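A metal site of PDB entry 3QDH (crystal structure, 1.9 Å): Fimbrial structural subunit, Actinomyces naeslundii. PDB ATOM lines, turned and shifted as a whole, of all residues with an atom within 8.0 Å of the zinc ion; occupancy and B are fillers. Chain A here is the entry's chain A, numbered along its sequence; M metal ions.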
ATOM      1  N   THR A  68     -18.380  -2.648   0.633  1.00  0.00           N
ATOM      2  CA  THR A  68     -19.592  -3.345   0.228  1.00  0.00           C
ATOM      3  C   THR A  68     -20.735  -2.332   0.209  1.00  0.00           C
ATOM      4  O   THR A  68     -21.108  -1.771   1.251  1.00  0.00           O
ATOM      5  CB  THR A  68     -19.922  -4.564   1.130  1.00  0.00           C
ATOM      6  OG1 THR A  68     -18.818  -5.470   1.129  1.00  0.00           O
ATOM      7  CG2 THR A  68     -21.150  -5.290   0.608  1.00  0.00           C
ATOM      8  N   LEU A  69     -21.243  -2.061  -0.994  1.00  0.00           N
ATOM      9  CA  LEU A  69     -22.375  -1.146  -1.185  1.00  0.00           C
ATOM     10  C   LEU A  69     -23.687  -1.771  -0.718  1.00  0.00           C
ATOM     11  O   LEU A  69     -23.792  -2.991  -0.637  1.00  0.00           O
ATOM     12  CB  LEU A  69     -22.518  -0.796  -2.678  1.00  0.00           C
ATOM     13  CG  LEU A  69     -21.362  -0.085  -3.383  1.00  0.00           C
ATOM     14  CD1 LEU A  69     -21.645  -0.043  -4.885  1.00  0.00           C
ATOM     15  CD2 LEU A  69     -21.128   1.335  -2.831  1.00  0.00           C
ATOM     16  N   ASP A  70     -24.668  -0.933  -0.415  1.00  0.00           N
ATOM     17  CA  ASP A  70     -26.005  -1.399  -0.148  1.00  0.00           C
ATOM     18  C   ASP A  70     -26.888  -1.002  -1.343  1.00  0.00           C
ATOM     19  O   ASP A  70     -26.499  -0.128  -2.135  1.00  0.00           O
ATOM     20  CB  ASP A  70     -26.528  -0.805   1.179  1.00  0.00           C
ATOM     21  CG  ASP A  70     -26.671   0.715   1.115  1.00  0.00           C
ATOM     22  OD1 ASP A  70     -27.501   1.203   0.318  1.00  0.00           O
ATOM     23  OD2 ASP A  70     -25.970   1.403   1.872  1.00  0.00           O
ATOM     24  N   PRO A  71     -28.067  -1.639  -1.484  1.00  0.00           N
ATOM     25  CA  PRO A  71     -28.931  -1.432  -2.646  1.00  0.00           C
ATOM     26  C   PRO A  71     -29.431   0.007  -2.840  1.00  0.00           C
ATOM     27  O   PRO A  71     -29.852   0.370  -3.952  1.00  0.00           O
ATOM     28  CB  PRO A  71     -30.117  -2.374  -2.375  1.00  0.00           C
ATOM     29  CG  PRO A  71     -29.578  -3.404  -1.467  1.00  0.00           C
ATOM     30  CD  PRO A  71     -28.625  -2.670  -0.587  1.00  0.00           C
ATOM     31  N   THR A  72     -29.366   0.832  -1.782  1.00  0.00           N
ATOM     32  CA  THR A  72     -29.786   2.236  -1.880  1.00  0.00           C
ATOM     33  C   THR A  72     -28.651   3.210  -2.247  1.00  0.00           C
ATOM     34  O   THR A  72     -28.833   4.433  -2.200  1.00  0.00           O
ATOM     35  CB  THR A  72     -30.526   2.736  -0.604  1.00  0.00           C
ATOM     36  OG1 THR A  72     -29.657   2.703   0.529  1.00  0.00           O
ATOM     37  CG2 THR A  72     -31.737   1.866  -0.322  1.00  0.00           C
ATOM     38  N   ASP A  73     -27.478   2.660  -2.615  1.00  0.00           N
ATOM     39  CA  ASP A  73     -26.307   3.461  -2.985  1.00  0.00           C
ATOM     40  C   ASP A  73     -26.311   3.956  -4.443  1.00  0.00           C
ATOM     41  O   ASP A  73     -25.582   4.871  -4.789  1.00  0.00           O
ATOM     42  CB  ASP A  73     -25.001   2.711  -2.662  1.00  0.00           C
ATOM     43  CG  ASP A  73     -24.695   2.707  -1.160  1.00  0.00           C
ATOM     44  OD1 ASP A  73     -25.200   3.629  -0.483  1.00  0.00           O
ATOM     45  OD2 ASP A  73     -23.978   1.811  -0.659  1.00  0.00           O
ATOM     46  N   TYR A  74     -27.167   3.351  -5.258  1.00  0.00           N
ATOM     47  CA  TYR A  74     -27.194   3.677  -6.688  1.00  0.00           C
ATOM     48  C   TYR A  74     -28.527   3.244  -7.278  1.00  0.00           C
ATOM     49  O   TYR A  74     -29.286   2.484  -6.675  1.00  0.00           O
ATOM     50  CB  TYR A  74     -26.049   2.952  -7.417  1.00  0.00           C
ATOM     51  CG  TYR A  74     -26.096   1.470  -7.168  1.00  0.00           C
ATOM     52  CD1 TYR A  74     -26.827   0.627  -8.001  1.00  0.00           C
ATOM     53  CD2 TYR A  74     -25.443   0.915  -6.058  1.00  0.00           C
ATOM     54  CE1 TYR A  74     -26.885  -0.744  -7.750  1.00  0.00           C
ATOM     55  CE2 TYR A  74     -25.508  -0.452  -5.800  1.00  0.00           C
ATOM     56  CZ  TYR A  74     -26.230  -1.268  -6.639  1.00  0.00           C
ATOM     57  OH  TYR A  74     -26.293  -2.616  -6.390  1.00  0.00           O
ATOM     58  N   THR A  88     -26.544   7.512  -5.572  1.00  0.00           N
ATOM     59  CA  THR A  88     -27.465   8.316  -4.780  1.00  0.00           C
ATOM     60  C   THR A  88     -26.642   9.179  -3.827  1.00  0.00           C
ATOM     61  O   THR A  88     -25.416   9.076  -3.784  1.00  0.00           O
ATOM     62  CB  THR A  88     -28.382   7.397  -3.943  1.00  0.00           C
ATOM     63  OG1 THR A  88     -27.558   6.594  -3.098  1.00  0.00           O
ATOM     64  CG2 THR A  88     -29.269   6.514  -4.842  1.00  0.00           C
ATOM     65  N   ALA A  89     -27.307   9.997  -3.008  1.00  0.00           N
ATOM     66  CA  ALA A  89     -26.574  10.829  -2.049  1.00  0.00           C
ATOM     67  C   ALA A  89     -25.599  10.034  -1.155  1.00  0.00           C
ATOM     68  O   ALA A  89     -24.449  10.422  -0.979  1.00  0.00           O
ATOM     69  CB  ALA A  89     -27.550  11.650  -1.199  1.00  0.00           C
ATOM     70  N   GLU A  90     -26.072   8.906  -0.614  1.00  0.00           N
ATOM     71  CA  GLU A  90     -25.250   8.009   0.223  1.00  0.00           C
ATOM     72  C   GLU A  90     -24.065   7.470  -0.569  1.00  0.00           C
ATOM     73  O   GLU A  90     -22.946   7.375  -0.056  1.00  0.00           O
ATOM     74  CB  GLU A  90     -26.056   6.776   0.626  1.00  0.00           C
ATOM     75  CG  GLU A  90     -26.905   6.858   1.822  1.00  0.00           C
ATOM     76  CD  GLU A  90     -27.897   5.679   1.844  1.00  0.00           C
ATOM     77  OE1 GLU A  90     -27.495   4.498   1.670  1.00  0.00           O
ATOM     78  OE2 GLU A  90     -29.081   5.962   2.038  1.00  0.00           O
ATOM     79  N   GLY A  91     -24.342   7.072  -1.796  1.00  0.00           N
ATOM     80  CA  GLY A  91     -23.300   6.562  -2.693  1.00  0.00           C
ATOM     81  C   GLY A  91     -22.234   7.597  -2.995  1.00  0.00           C
ATOM     82  O   GLY A  91     -21.054   7.288  -3.046  1.00  0.00           O
ATOM     83  N   LEU A  92     -22.652   8.846  -3.200  1.00  0.00           N
ATOM     84  CA  LEU A  92     -21.691   9.912  -3.514  1.00  0.00           C
ATOM     85  C   LEU A  92     -20.786  10.207  -2.336  1.00  0.00           C
ATOM     86  O   LEU A  92     -19.609  10.485  -2.519  1.00  0.00           O
ATOM     87  CB  LEU A  92     -22.408  11.208  -3.937  1.00  0.00           C
ATOM     88  CG  LEU A  92     -23.254  11.115  -5.215  1.00  0.00           C
ATOM     89  CD1 LEU A  92     -23.966  12.467  -5.457  1.00  0.00           C
ATOM     90  CD2 LEU A  92     -22.384  10.734  -6.420  1.00  0.00           C
ATOM     91  N   ARG A  94     -19.890   7.914  -0.105  1.00  0.00           N
ATOM     92  CA  ARG A  94     -18.926   6.786  -0.147  1.00  0.00           C
ATOM     93  C   ARG A  94     -17.769   6.990  -1.122  1.00  0.00           C
ATOM     94  O   ARG A  94     -16.588   6.721  -0.809  1.00  0.00           O
ATOM     95  CB  ARG A  94     -19.644   5.496  -0.532  1.00  0.00           C
ATOM     96  CG  ARG A  94     -20.528   4.861   0.550  1.00  0.00           C
ATOM     97  CD  ARG A  94     -20.919   3.482   0.049  1.00  0.00           C
ATOM     98  NE  ARG A  94     -21.985   2.810   0.818  1.00  0.00           N
ATOM     99  CZ  ARG A  94     -21.771   2.065   1.900  1.00  0.00           C
ATOM    100  NH1 ARG A  94     -20.543   1.907   2.358  1.00  0.00           N
ATOM    101  NH2 ARG A  94     -22.784   1.478   2.523  1.00  0.00           N
HETATM  102 ZN    ZN M   1     -25.890   3.375   1.415  1.00  0.00          ZN
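OE1 of Glu 90 lies close to OG1 of Thr 72, 3.0 Å away. NH2 of Arg 94 lies close to OD2 of Asp 70, 3.3 Å away. OD1 of Asp 70 sits at hydrogen-bond distance from OG1 of Thr 72 (2.6 Å). The side-chain carboxylate (OD2) of Asp 73 is in salt-bridge range of the guanidinium group (NE) of Arg 94, 2.7 Å away. The backbone carbonyl oxygen (O) of Asp 73 lies within hydrogen-bond range of the backbone NH (N) of Thr 88 (2.9 Å). The side-chain hydroxyl (OG1) of Thr 88 is in hydrogen-bond range of the backbone carbonyl oxygen (O) of Thr 72, 2.7 Å away.
OG1 of Thr 72 touches the zinc ion, 3.9 Å away. NH2 of Arg 94 touches the zinc ion, at 3.8 Å. The nearest printed residue that does not touch the zinc ion is Gly 91 (5.1 Å).
The side-chain carboxylate (OE1) of Glu 90 binds the zinc ion (2.0 Å). OD2 of Asp 70 binds the zinc ion. OD1 of Asp 73 is bound to the zinc ion (2.0 Å).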
